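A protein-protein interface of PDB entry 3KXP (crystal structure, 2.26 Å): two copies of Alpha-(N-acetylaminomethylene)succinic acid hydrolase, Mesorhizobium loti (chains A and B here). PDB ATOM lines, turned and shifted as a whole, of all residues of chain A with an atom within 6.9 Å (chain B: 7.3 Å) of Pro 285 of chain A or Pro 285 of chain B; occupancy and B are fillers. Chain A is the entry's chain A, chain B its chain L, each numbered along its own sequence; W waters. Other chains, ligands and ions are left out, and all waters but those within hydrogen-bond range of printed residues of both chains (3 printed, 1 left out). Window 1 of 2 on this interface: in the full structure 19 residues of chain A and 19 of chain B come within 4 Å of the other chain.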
ATOM      1  N   PRO A 257      -8.787   2.753  18.656  1.00  0.00           N
ATOM      2  CA  PRO A 257      -7.740   3.727  18.311  1.00  0.00           C
ATOM      3  C   PRO A 257      -8.127   4.656  17.163  1.00  0.00           C
ATOM      4  O   PRO A 257      -8.629   4.207  16.132  1.00  0.00           O
ATOM      5  CB  PRO A 257      -6.551   2.842  17.939  1.00  0.00           C
ATOM      6  CG  PRO A 257      -6.780   1.608  18.770  1.00  0.00           C
ATOM      7  CD  PRO A 257      -8.259   1.379  18.599  1.00  0.00           C
ATOM      8  N   VAL A 258      -7.886   5.948  17.352  1.00  0.00           N
ATOM      9  CA  VAL A 258      -8.180   6.939  16.327  1.00  0.00           C
ATOM     10  C   VAL A 258      -7.039   7.944  16.198  1.00  0.00           C
ATOM     11  O   VAL A 258      -6.671   8.611  17.162  1.00  0.00           O
ATOM     12  CB  VAL A 258      -9.480   7.704  16.641  1.00  0.00           C
ATOM     13  CG1 VAL A 258      -9.722   8.797  15.589  1.00  0.00           C
ATOM     14  CG2 VAL A 258     -10.650   6.728  16.678  1.00  0.00           C
ATOM     15  N   LEU A 259      -6.464   8.029  15.006  1.00  0.00           N
ATOM     16  CA  LEU A 259      -5.393   8.972  14.747  1.00  0.00           C
ATOM     17  C   LEU A 259      -6.045  10.198  14.109  1.00  0.00           C
ATOM     18  O   LEU A 259      -6.753  10.078  13.112  1.00  0.00           O
ATOM     19  CB  LEU A 259      -4.376   8.376  13.782  1.00  0.00           C
ATOM     20  CG  LEU A 259      -3.286   9.339  13.294  1.00  0.00           C
ATOM     21  CD1 LEU A 259      -2.280   9.604  14.417  1.00  0.00           C
ATOM     22  CD2 LEU A 259      -2.567   8.727  12.089  1.00  0.00           C
ATOM     23  N   ILE A 260      -5.825  11.370  14.687  1.00  0.00           N
ATOM     24  CA  ILE A 260      -6.407  12.585  14.136  1.00  0.00           C
ATOM     25  C   ILE A 260      -5.371  13.282  13.268  1.00  0.00           C
ATOM     26  O   ILE A 260      -4.265  13.584  13.724  1.00  0.00           O
ATOM     27  CB  ILE A 260      -6.846  13.559  15.242  1.00  0.00           C
ATOM     28  CG1 ILE A 260      -7.856  12.884  16.170  1.00  0.00           C
ATOM     29  CG2 ILE A 260      -7.467  14.795  14.619  1.00  0.00           C
ATOM     30  CD1 ILE A 260      -8.223  13.725  17.386  1.00  0.00           C
ATOM     31  N   VAL A 261      -5.722  13.520  12.010  1.00  0.00           N
ATOM     32  CA  VAL A 261      -4.813  14.194  11.098  1.00  0.00           C
ATOM     33  C   VAL A 261      -5.446  15.494  10.642  1.00  0.00           C
ATOM     34  O   VAL A 261      -6.591  15.501  10.184  1.00  0.00           O
ATOM     35  CB  VAL A 261      -4.502  13.329   9.859  1.00  0.00           C
ATOM     36  CG1 VAL A 261      -3.636  14.109   8.891  1.00  0.00           C
ATOM     37  CG2 VAL A 261      -3.785  12.055  10.284  1.00  0.00           C
ATOM     38  N   SER A 278      -8.831  17.695  20.999  1.00  0.00           N
ATOM     39  CA  SER A 278      -7.793  17.078  21.816  1.00  0.00           C
ATOM     40  C   SER A 278      -8.083  17.206  23.307  1.00  0.00           C
ATOM     41  O   SER A 278      -7.716  16.343  24.085  1.00  0.00           O
ATOM     42  CB  SER A 278      -6.424  17.686  21.504  1.00  0.00           C
ATOM     43  OG  SER A 278      -5.911  17.156  20.294  1.00  0.00           O
ATOM     44  N   ARG A 281     -10.648  14.519  23.973  1.00  0.00           N
ATOM     45  CA  ARG A 281     -10.006  13.209  23.942  1.00  0.00           C
ATOM     46  C   ARG A 281      -8.500  13.406  23.869  1.00  0.00           C
ATOM     47  O   ARG A 281      -7.889  13.255  22.812  1.00  0.00           O
ATOM     48  CB  ARG A 281     -10.477  12.393  22.728  1.00  0.00           C
ATOM     49  CG  ARG A 281     -11.928  11.918  22.805  1.00  0.00           C
ATOM     50  CD  ARG A 281     -12.144  11.009  24.009  1.00  0.00           C
ATOM     51  NE  ARG A 281     -11.260   9.847  23.990  1.00  0.00           N
ATOM     52  CZ  ARG A 281     -11.499   8.732  23.305  1.00  0.00           C
ATOM     53  NH1 ARG A 281     -10.636   7.727  23.348  1.00  0.00           N
ATOM     54  NH2 ARG A 281     -12.608   8.616  22.590  1.00  0.00           N
ATOM     55  N   PRO A 282      -7.879  13.759  24.995  1.00  0.00           N
ATOM     56  CA  PRO A 282      -6.430  13.965  24.990  1.00  0.00           C
ATOM     57  C   PRO A 282      -5.613  12.731  24.652  1.00  0.00           C
ATOM     58  O   PRO A 282      -4.464  12.845  24.233  1.00  0.00           O
ATOM     59  CB  PRO A 282      -6.151  14.491  26.397  1.00  0.00           C
ATOM     60  CG  PRO A 282      -7.305  13.959  27.217  1.00  0.00           C
ATOM     61  CD  PRO A 282      -8.468  14.116  26.297  1.00  0.00           C
ATOM     62  N   ASP A 283      -6.210  11.554  24.805  1.00  0.00           N
ATOM     63  CA  ASP A 283      -5.501  10.303  24.539  1.00  0.00           C
ATOM     64  C   ASP A 283      -5.344   9.935  23.061  1.00  0.00           C
ATOM     65  O   ASP A 283      -4.517   9.090  22.722  1.00  0.00           O
ATOM     66  CB  ASP A 283      -6.207   9.160  25.268  1.00  0.00           C
ATOM     67  CG  ASP A 283      -7.623   8.945  24.760  1.00  0.00           C
ATOM     68  OD1 ASP A 283      -7.860   7.957  24.023  1.00  0.00           O
ATOM     69  OD2 ASP A 283      -8.496   9.779  25.082  1.00  0.00           O
ATOM     70  N   LEU A 284      -6.131  10.549  22.183  1.00  0.00           N
ATOM     71  CA  LEU A 284      -6.042  10.227  20.760  1.00  0.00           C
ATOM     72  C   LEU A 284      -4.835  10.898  20.092  1.00  0.00           C
ATOM     73  O   LEU A 284      -4.736  12.124  20.064  1.00  0.00           O
ATOM     74  CB  LEU A 284      -7.340  10.638  20.049  1.00  0.00           C
ATOM     75  CG  LEU A 284      -8.606   9.917  20.529  1.00  0.00           C
ATOM     76  CD1 LEU A 284      -9.858  10.486  19.838  1.00  0.00           C
ATOM     77  CD2 LEU A 284      -8.461   8.417  20.247  1.00  0.00           C
ATOM     78  N   PRO A 285      -3.898  10.099  19.552  1.00  0.00           N
ATOM     79  CA  PRO A 285      -2.708  10.657  18.891  1.00  0.00           C
ATOM     80  C   PRO A 285      -3.064  11.647  17.787  1.00  0.00           C
ATOM     81  O   PRO A 285      -4.027  11.454  17.050  1.00  0.00           O
ATOM     82  CB  PRO A 285      -1.991   9.421  18.353  1.00  0.00           C
ATOM     83  CG  PRO A 285      -3.121   8.474  18.094  1.00  0.00           C
ATOM     84  CD  PRO A 285      -3.970   8.645  19.346  1.00  0.00           C
ATOM     85  N   VAL A 286      -2.270  12.703  17.677  1.00  0.00           N
ATOM     86  CA  VAL A 286      -2.515  13.745  16.692  1.00  0.00           C
ATOM     87  C   VAL A 286      -1.329  14.013  15.769  1.00  0.00           C
ATOM     88  O   VAL A 286      -0.171  13.986  16.199  1.00  0.00           O
ATOM     89  CB  VAL A 286      -2.889  15.073  17.398  1.00  0.00           C
ATOM     90  CG1 VAL A 286      -3.072  16.166  16.376  1.00  0.00           C
ATOM     91  CG2 VAL A 286      -4.171  14.894  18.223  1.00  0.00           C
ATOM     92  N   VAL A 287      -1.645  14.288  14.504  1.00  0.00           N
ATOM     93  CA  VAL A 287      -0.665  14.607  13.469  1.00  0.00           C
ATOM     94  C   VAL A 287      -1.162  15.852  12.716  1.00  0.00           C
ATOM     95  O   VAL A 287      -2.302  15.882  12.252  1.00  0.00           O
ATOM     96  CB  VAL A 287      -0.505  13.431  12.466  1.00  0.00           C
ATOM     97  CG1 VAL A 287       0.161  13.904  11.185  1.00  0.00           C
ATOM     98  CG2 VAL A 287       0.331  12.321  13.092  1.00  0.00           C
ATOM     99  N   LYS A 306       3.481   8.102   5.825  1.00  0.00           N
ATOM    100  CA  LYS A 306       4.314   7.857   7.001  1.00  0.00           C
ATOM    101  C   LYS A 306       3.514   7.934   8.311  1.00  0.00           C
ATOM    102  O   LYS A 306       3.766   7.189   9.256  1.00  0.00           O
ATOM    103  CB  LYS A 306       5.466   8.862   7.042  1.00  0.00           C
ATOM    104  CG  LYS A 306       6.847   8.234   6.982  1.00  0.00           C
ATOM    105  CD  LYS A 306       7.064   7.229   8.112  1.00  0.00           C
ATOM    106  CE  LYS A 306       8.478   6.662   8.098  1.00  0.00           C
ATOM    107  NZ  LYS A 306       8.708   5.693   9.211  1.00  0.00           N
ATOM    108  N   ALA A 307       2.552   8.845   8.359  1.00  0.00           N
ATOM    109  CA  ALA A 307       1.726   9.013   9.542  1.00  0.00           C
ATOM    110  C   ALA A 307       0.857   7.785   9.734  1.00  0.00           C
ATOM    111  O   ALA A 307       0.612   7.363  10.861  1.00  0.00           O
ATOM    112  CB  ALA A 307       0.861  10.242   9.400  1.00  0.00           C
ATOM    113  N   ASN A 310       3.147   4.856  10.782  1.00  0.00           N
ATOM    114  CA  ASN A 310       3.620   5.012  12.159  1.00  0.00           C
ATOM    115  C   ASN A 310       2.510   4.561  13.105  1.00  0.00           C
ATOM    116  O   ASN A 310       2.761   3.930  14.132  1.00  0.00           O
ATOM    117  CB  ASN A 310       3.972   6.469  12.476  1.00  0.00           C
ATOM    118  CG  ASN A 310       5.307   6.897  11.889  1.00  0.00           C
ATOM    119  OD1 ASN A 310       6.223   6.083  11.730  1.00  0.00           O
ATOM    120  ND2 ASN A 310       5.431   8.188  11.585  1.00  0.00           N
ATOM    121  N   PHE A 311       1.277   4.883  12.723  1.00  0.00           N
ATOM    122  CA  PHE A 311       0.089   4.562  13.507  1.00  0.00           C
ATOM    123  C   PHE A 311      -0.189   3.071  13.639  1.00  0.00           C
ATOM    124  O   PHE A 311      -0.125   2.518  14.734  1.00  0.00           O
ATOM    125  CB  PHE A 311      -1.136   5.236  12.885  1.00  0.00           C
ATOM    126  CG  PHE A 311      -2.379   5.144  13.726  1.00  0.00           C
ATOM    127  CD1 PHE A 311      -3.605   4.844  13.142  1.00  0.00           C
ATOM    128  CD2 PHE A 311      -2.332   5.398  15.095  1.00  0.00           C
ATOM    129  CE1 PHE A 311      -4.769   4.800  13.906  1.00  0.00           C
ATOM    130  CE2 PHE A 311      -3.484   5.358  15.871  1.00  0.00           C
ATOM    131  CZ  PHE A 311      -4.709   5.059  15.279  1.00  0.00           C
ATOM    132  N   VAL B 162       8.367   3.102  19.868  1.00  0.00           N
ATOM    133  CA  VAL B 162       8.782   3.853  21.039  1.00  0.00           C
ATOM    134  C   VAL B 162       7.742   4.857  21.504  1.00  0.00           C
ATOM    135  O   VAL B 162       7.130   5.573  20.701  1.00  0.00           O
ATOM    136  CB  VAL B 162      10.085   4.644  20.779  1.00  0.00           C
ATOM    137  CG1 VAL B 162      10.402   5.521  21.991  1.00  0.00           C
ATOM    138  CG2 VAL B 162      11.233   3.696  20.483  1.00  0.00           C
ATOM    139  N   PRO B 257       8.181   3.604  14.463  1.00  0.00           N
ATOM    140  CA  PRO B 257       7.144   4.479  15.025  1.00  0.00           C
ATOM    141  C   PRO B 257       7.520   5.084  16.385  1.00  0.00           C
ATOM    142  O   PRO B 257       8.074   4.398  17.247  1.00  0.00           O
ATOM    143  CB  PRO B 257       5.930   3.556  15.136  1.00  0.00           C
ATOM    144  CG  PRO B 257       6.171   2.531  14.064  1.00  0.00           C
ATOM    145  CD  PRO B 257       7.645   2.258  14.195  1.00  0.00           C
ATOM    146  N   VAL B 258       7.225   6.372  16.559  1.00  0.00           N
ATOM    147  CA  VAL B 258       7.491   7.065  17.811  1.00  0.00           C
ATOM    148  C   VAL B 258       6.292   7.929  18.199  1.00  0.00           C
ATOM    149  O   VAL B 258       5.820   8.752  17.404  1.00  0.00           O
ATOM    150  CB  VAL B 258       8.734   7.987  17.729  1.00  0.00           C
ATOM    151  CG1 VAL B 258       8.904   8.720  19.049  1.00  0.00           C
ATOM    152  CG2 VAL B 258       9.991   7.175  17.434  1.00  0.00           C
ATOM    153  N   LEU B 259       5.792   7.715  19.416  1.00  0.00           N
ATOM    154  CA  LEU B 259       4.675   8.485  19.949  1.00  0.00           C
ATOM    155  C   LEU B 259       5.258   9.530  20.899  1.00  0.00           C
ATOM    156  O   LEU B 259       5.867   9.185  21.921  1.00  0.00           O
ATOM    157  CB  LEU B 259       3.697   7.595  20.721  1.00  0.00           C
ATOM    158  CG  LEU B 259       2.534   8.372  21.360  1.00  0.00           C
ATOM    159  CD1 LEU B 259       1.612   8.905  20.261  1.00  0.00           C
ATOM    160  CD2 LEU B 259       1.741   7.465  22.307  1.00  0.00           C
ATOM    161  N   ILE B 260       5.080  10.803  20.556  1.00  0.00           N
ATOM    162  CA  ILE B 260       5.596  11.878  21.381  1.00  0.00           C
ATOM    163  C   ILE B 260       4.528  12.320  22.361  1.00  0.00           C
ATOM    164  O   ILE B 260       3.440  12.734  21.953  1.00  0.00           O
ATOM    165  CB  ILE B 260       6.006  13.072  20.532  1.00  0.00           C
ATOM    166  CG1 ILE B 260       7.024  12.628  19.482  1.00  0.00           C
ATOM    167  CG2 ILE B 260       6.579  14.151  21.409  1.00  0.00           C
ATOM    168  CD1 ILE B 260       7.393  13.715  18.489  1.00  0.00           C
ATOM    169  N   VAL B 261       4.840  12.225  23.651  1.00  0.00           N
ATOM    170  CA  VAL B 261       3.911  12.612  24.704  1.00  0.00           C
ATOM    171  C   VAL B 261       4.459  13.760  25.550  1.00  0.00           C
ATOM    172  O   VAL B 261       5.557  13.668  26.092  1.00  0.00           O
ATOM    173  CB  VAL B 261       3.617  11.432  25.648  1.00  0.00           C
ATOM    174  CG1 VAL B 261       2.606  11.857  26.706  1.00  0.00           C
ATOM    175  CG2 VAL B 261       3.091  10.245  24.851  1.00  0.00           C
ATOM    176  N   SER B 278       7.825  18.804  16.132  1.00  0.00           N
ATOM    177  CA  SER B 278       6.826  18.394  15.151  1.00  0.00           C
ATOM    178  C   SER B 278       7.105  18.895  13.737  1.00  0.00           C
ATOM    179  O   SER B 278       6.666  18.279  12.771  1.00  0.00           O
ATOM    180  CB  SER B 278       5.420  18.821  15.589  1.00  0.00           C
ATOM    181  OG  SER B 278       4.910  17.906  16.543  1.00  0.00           O
ATOM    182  N   ARG B 281       9.726  16.404  12.507  1.00  0.00           N
ATOM    183  CA  ARG B 281       9.126  15.115  12.204  1.00  0.00           C
ATOM    184  C   ARG B 281       7.608  15.194  12.321  1.00  0.00           C
ATOM    185  O   ARG B 281       7.025  14.639  13.251  1.00  0.00           O
ATOM    186  CB  ARG B 281       9.658  14.047  13.171  1.00  0.00           C
ATOM    187  CG  ARG B 281      11.099  13.625  12.935  1.00  0.00           C
ATOM    188  CD  ARG B 281      11.254  12.980  11.560  1.00  0.00           C
ATOM    189  NE  ARG B 281      10.385  11.814  11.384  1.00  0.00           N
ATOM    190  CZ  ARG B 281      10.752  10.548  11.592  1.00  0.00           C
ATOM    191  NH1 ARG B 281      11.989  10.255  11.986  1.00  0.00           N
ATOM    192  NH2 ARG B 281       9.875   9.566  11.411  1.00  0.00           N
ATOM    193  N   PRO B 282       6.945  15.865  11.365  1.00  0.00           N
ATOM    194  CA  PRO B 282       5.482  16.004  11.390  1.00  0.00           C
ATOM    195  C   PRO B 282       4.694  14.698  11.305  1.00  0.00           C
ATOM    196  O   PRO B 282       3.492  14.666  11.593  1.00  0.00           O
ATOM    197  CB  PRO B 282       5.203  16.923  10.202  1.00  0.00           C
ATOM    198  CG  PRO B 282       6.308  16.571   9.237  1.00  0.00           C
ATOM    199  CD  PRO B 282       7.512  16.484  10.150  1.00  0.00           C
ATOM    200  N   ASP B 283       5.366  13.619  10.923  1.00  0.00           N
ATOM    201  CA  ASP B 283       4.707  12.325  10.791  1.00  0.00           C
ATOM    202  C   ASP B 283       4.531  11.586  12.123  1.00  0.00           C
ATOM    203  O   ASP B 283       3.644  10.735  12.260  1.00  0.00           O
ATOM    204  CB  ASP B 283       5.501  11.455   9.828  1.00  0.00           C
ATOM    205  CG  ASP B 283       6.907  11.221  10.303  1.00  0.00           C
ATOM    206  OD1 ASP B 283       7.216  10.080  10.688  1.00  0.00           O
ATOM    207  OD2 ASP B 283       7.703  12.181  10.309  1.00  0.00           O
ATOM    208  N   LEU B 284       5.375  11.901  13.102  1.00  0.00           N
ATOM    209  CA  LEU B 284       5.277  11.246  14.402  1.00  0.00           C
ATOM    210  C   LEU B 284       4.041  11.729  15.164  1.00  0.00           C
ATOM    211  O   LEU B 284       3.865  12.928  15.399  1.00  0.00           O
ATOM    212  CB  LEU B 284       6.547  11.503  15.221  1.00  0.00           C
ATOM    213  CG  LEU B 284       7.852  11.056  14.537  1.00  0.00           C
ATOM    214  CD1 LEU B 284       9.021  11.330  15.456  1.00  0.00           C
ATOM    215  CD2 LEU B 284       7.793   9.574  14.185  1.00  0.00           C
ATOM    216  N   PRO B 285       3.156  10.796  15.546  1.00  0.00           N
ATOM    217  CA  PRO B 285       1.943  11.162  16.282  1.00  0.00           C
ATOM    218  C   PRO B 285       2.268  11.828  17.634  1.00  0.00           C
ATOM    219  O   PRO B 285       3.249  11.477  18.301  1.00  0.00           O
ATOM    220  CB  PRO B 285       1.209   9.826  16.418  1.00  0.00           C
ATOM    221  CG  PRO B 285       2.333   8.822  16.445  1.00  0.00           C
ATOM    222  CD  PRO B 285       3.252   9.336  15.372  1.00  0.00           C
ATOM    223  N   VAL B 286       1.438  12.792  18.022  1.00  0.00           N
ATOM    224  CA  VAL B 286       1.635  13.542  19.253  1.00  0.00           C
ATOM    225  C   VAL B 286       0.457  13.474  20.215  1.00  0.00           C
ATOM    226  O   VAL B 286      -0.701  13.483  19.794  1.00  0.00           O
ATOM    227  CB  VAL B 286       1.875  15.033  18.941  1.00  0.00           C
ATOM    228  CG1 VAL B 286       2.003  15.828  20.233  1.00  0.00           C
ATOM    229  CG2 VAL B 286       3.123  15.194  18.081  1.00  0.00           C
ATOM    230  N   VAL B 287       0.771  13.412  21.507  1.00  0.00           N
ATOM    231  CA  VAL B 287      -0.232  13.399  22.567  1.00  0.00           C
ATOM    232  C   VAL B 287       0.185  14.429  23.620  1.00  0.00           C
ATOM    233  O   VAL B 287       1.299  14.376  24.144  1.00  0.00           O
ATOM    234  CB  VAL B 287      -0.351  12.012  23.257  1.00  0.00           C
ATOM    235  CG1 VAL B 287      -1.126  12.143  24.556  1.00  0.00           C
ATOM    236  CG2 VAL B 287      -1.077  11.035  22.350  1.00  0.00           C
ATOM    237  N   VAL B 288      -0.704  15.372  23.910  1.00  0.00           N
ATOM    238  CA  VAL B 288      -0.440  16.401  24.908  1.00  0.00           C
ATOM    239  C   VAL B 288      -1.422  16.168  26.043  1.00  0.00           C
ATOM    240  O   VAL B 288      -2.632  16.230  25.836  1.00  0.00           O
ATOM    241  CB  VAL B 288      -0.655  17.810  24.332  1.00  0.00           C
ATOM    242  CG1 VAL B 288      -0.511  18.850  25.435  1.00  0.00           C
ATOM    243  CG2 VAL B 288       0.345  18.077  23.219  1.00  0.00           C
ATOM    244  N   LYS B 306      -4.149   4.864  28.218  1.00  0.00           N
ATOM    245  CA  LYS B 306      -4.996   4.950  27.038  1.00  0.00           C
ATOM    246  C   LYS B 306      -4.207   5.390  25.796  1.00  0.00           C
ATOM    247  O   LYS B 306      -4.397   4.835  24.709  1.00  0.00           O
ATOM    248  CB  LYS B 306      -6.147   5.926  27.294  1.00  0.00           C
ATOM    249  CG  LYS B 306      -7.540   5.340  27.086  1.00  0.00           C
ATOM    250  CD  LYS B 306      -7.753   4.846  25.663  1.00  0.00           C
ATOM    251  CE  LYS B 306      -9.175   4.330  25.466  1.00  0.00           C
ATOM    252  NZ  LYS B 306      -9.377   3.704  24.130  1.00  0.00           N
ATOM    253  N   ALA B 307      -3.325   6.378  25.957  1.00  0.00           N
ATOM    254  CA  ALA B 307      -2.525   6.859  24.834  1.00  0.00           C
ATOM    255  C   ALA B 307      -1.601   5.760  24.351  1.00  0.00           C
ATOM    256  O   ALA B 307      -1.370   5.616  23.156  1.00  0.00           O
ATOM    257  CB  ALA B 307      -1.711   8.081  25.226  1.00  0.00           C
ATOM    258  N   ASN B 310      -3.766   3.159  22.353  1.00  0.00           N
ATOM    259  CA  ASN B 310      -4.272   3.639  21.070  1.00  0.00           C
ATOM    260  C   ASN B 310      -3.169   3.519  20.027  1.00  0.00           C
ATOM    261  O   ASN B 310      -3.425   3.245  18.853  1.00  0.00           O
ATOM    262  CB  ASN B 310      -4.715   5.107  21.148  1.00  0.00           C
ATOM    263  CG  ASN B 310      -6.004   5.289  21.920  1.00  0.00           C
ATOM    264  OD1 ASN B 310      -6.908   4.458  21.846  1.00  0.00           O
ATOM    265  ND2 ASN B 310      -6.104   6.390  22.655  1.00  0.00           N
ATOM    266  N   PHE B 311      -1.941   3.724  20.485  1.00  0.00           N
ATOM    267  CA  PHE B 311      -0.749   3.685  19.648  1.00  0.00           C
ATOM    268  C   PHE B 311      -0.333   2.274  19.207  1.00  0.00           C
ATOM    269  O   PHE B 311      -0.186   2.009  18.016  1.00  0.00           O
ATOM    270  CB  PHE B 311       0.400   4.360  20.412  1.00  0.00           C
ATOM    271  CG  PHE B 311       1.685   4.455  19.646  1.00  0.00           C
ATOM    272  CD1 PHE B 311       2.865   3.952  20.187  1.00  0.00           C
ATOM    273  CD2 PHE B 311       1.734   5.087  18.409  1.00  0.00           C
ATOM    274  CE1 PHE B 311       4.079   4.081  19.504  1.00  0.00           C
ATOM    275  CE2 PHE B 311       2.940   5.223  17.720  1.00  0.00           C
ATOM    276  CZ  PHE B 311       4.114   4.719  18.271  1.00  0.00           C
ATOM    277  N   ALA B 314      -3.321   0.113  17.235  1.00  0.00           N
ATOM    278  CA  ALA B 314      -3.888   0.646  15.996  1.00  0.00           C
ATOM    279  C   ALA B 314      -3.883  -0.379  14.860  1.00  0.00           C
ATOM    280  O   ALA B 314      -2.922  -1.136  14.696  1.00  0.00           O
ATOM    281  CB  ALA B 314      -3.135   1.915  15.570  1.00  0.00           C
HETATM  282  O   HOH W   1      -3.597  15.054  22.634  1.00  0.00           O
HETATM  283  O   HOH W   2      -9.811   4.974  21.862  1.00  0.00           O
HETATM  284  O   HOH W   3       9.103   6.511  12.201  1.00  0.00           O
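Printed residues of chain B within 4 Å of Pro 257 of chain A: Asn 310 (3.3 Å) and Ala 314 (3.96 Å). Of chain B, only Pro 285, Val 286 and Val 287 come within 4 Å of Pro 285 of chain A. Of the printed residues of chain B, Asn 310 of chain A touches Pro 257, Asp 283, Leu 284 and Phe 311. Of the printed residues of chain A, Pro 282 of chain B touches Val 287. Of the printed residues of chain A, Leu 284 of chain B touches Asn 310 (3.8 Å). Pro 285 of chain B touches three residues of chain A. The nearest printed residue of chain A that does not touch Pro 282 of chain B is Ala 307 of chain A (5.6 Å).
Pro 282 of chain A touches Val 287 of chain B (O to CG1, 3.4 Å). Val 287 of chain B touches Asp 283 of chain A. Pro 285 of chain B touches Pro 285 of chain A. Pro 285 of chain A touches Val 286 of chain B (CA to O, 3.6 Å). Val 287 of chain B touches Pro 285 of chain A. O of Val 286 of chain A touches CA of Pro 285 of chain B (3.5 Å). Val 287 of chain A touches Pro 282 of chain B. Val 287 of chain A touches Pro 285 of chain B (CG2 to CA, 3.8 Å). Phe 311 of chain A touches Asn 310 of chain B. Phe 311 of chain A touches Ala 314 of chain B (O to CB, 3.2 Å).
The backbone carbonyl oxygen (O) of Pro 257 of chain B sits at hydrogen-bond distance from the backbone NH (N) of Val 162 of chain B, at 2.9 Å. O of Pro 285 of chain B is in hydrogen-bond range of N of Ile 260 of chain B, at 3.0 Å. The backbone carbonyl oxygen (O) of Lys 306 of chain B sits at hydrogen-bond distance from the side-chain amide nitrogen (ND2) of Asn 310 of chain B, at 3.1 Å. NH2 of Arg 281 of chain B lies within salt-bridge range of OD1 of Asp 283 of chain B (2.8 Å). The backbone carbonyl oxygen (O) of Ile 260 of chain A lies within hydrogen-bond range of the backbone NH (N) of Val 287 of chain A. The backbone NH (N) of Val 287 of chain B lies within hydrogen-bond range of the backbone carbonyl oxygen (O) of Ile 260 of chain B, 2.8 Å away.
Of the 17 printed residues of chain A, 11 touch a printed residue of chain B. Among the printed residues, 26 pairs touch across the chains. Among the printed residues, no Asp or Glu carboxylate lies within 4 Å of a Lys or Arg side-chain nitrogen of the other chain.
The side-chain amide nitrogen (ND2) of Asn 310 of chain B sits at hydrogen-bond distance from the side-chain carboxylate (OD1) of Asp 283 of chain A (2.7 Å). OD1 of Asp 283 of chain B sits at hydrogen-bond distance from ND2 of Asn 310 of chain A (2.8 Å). O of Phe 311 of chain A lies close to O of Phe 311 of chain B, 3.3 Å away. N of Val 286 of chain B lies within hydrogen-bond range of O of Val 286 of chain A, at 2.7 Å.
Water W2 lies within hydrogen-bond range of the side-chain amino group of Lys 306 of chain B (2.6 Å), the side-chain amide oxygen of Asn 310 of chain B (2.9 Å) and the guanidinium group of Arg 281 of chain A (3.2 Å). Water W1 bridges O of Pro 282 of chain A (2.9 Å) and N of Val 288 of chain B (3.2 Å). Water W3 lies within hydrogen-bond range of the side-chain amide oxygen of Asn 310 of chain A (2.9 Å), the side-chain amino group of Lys 306 of chain A (3.1 Å) and the guanidinium group of Arg 281 of chain B (3.2 Å).
Asp 283 of chain A touches Lys 306 of chain B, and with the chains exchanged Lys 306 of chain A touches Asp 283 of chain B. Asp 283 of chain A touches Ala 307 of chain B, and with the chains exchanged Ala 307 of chain A touches Asp 283 of chain B. Pro 285 of chain A touches Val 287 of chain B, and with the chains exchanged Val 287 of chain A touches Pro 285 of chain B. Val 286 of chain A touches its own counterpart, Val 286 of chain B. Positions printed for both chains: 257, 258, 259, 260, 261, 278, 281, 282, 283, 284, 285, 286, 287, 306, 307, 310 and 311. Of the 26 pairs that touch across the chains among the printed residues, 23 have their exchanged pair printed and touching as well.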
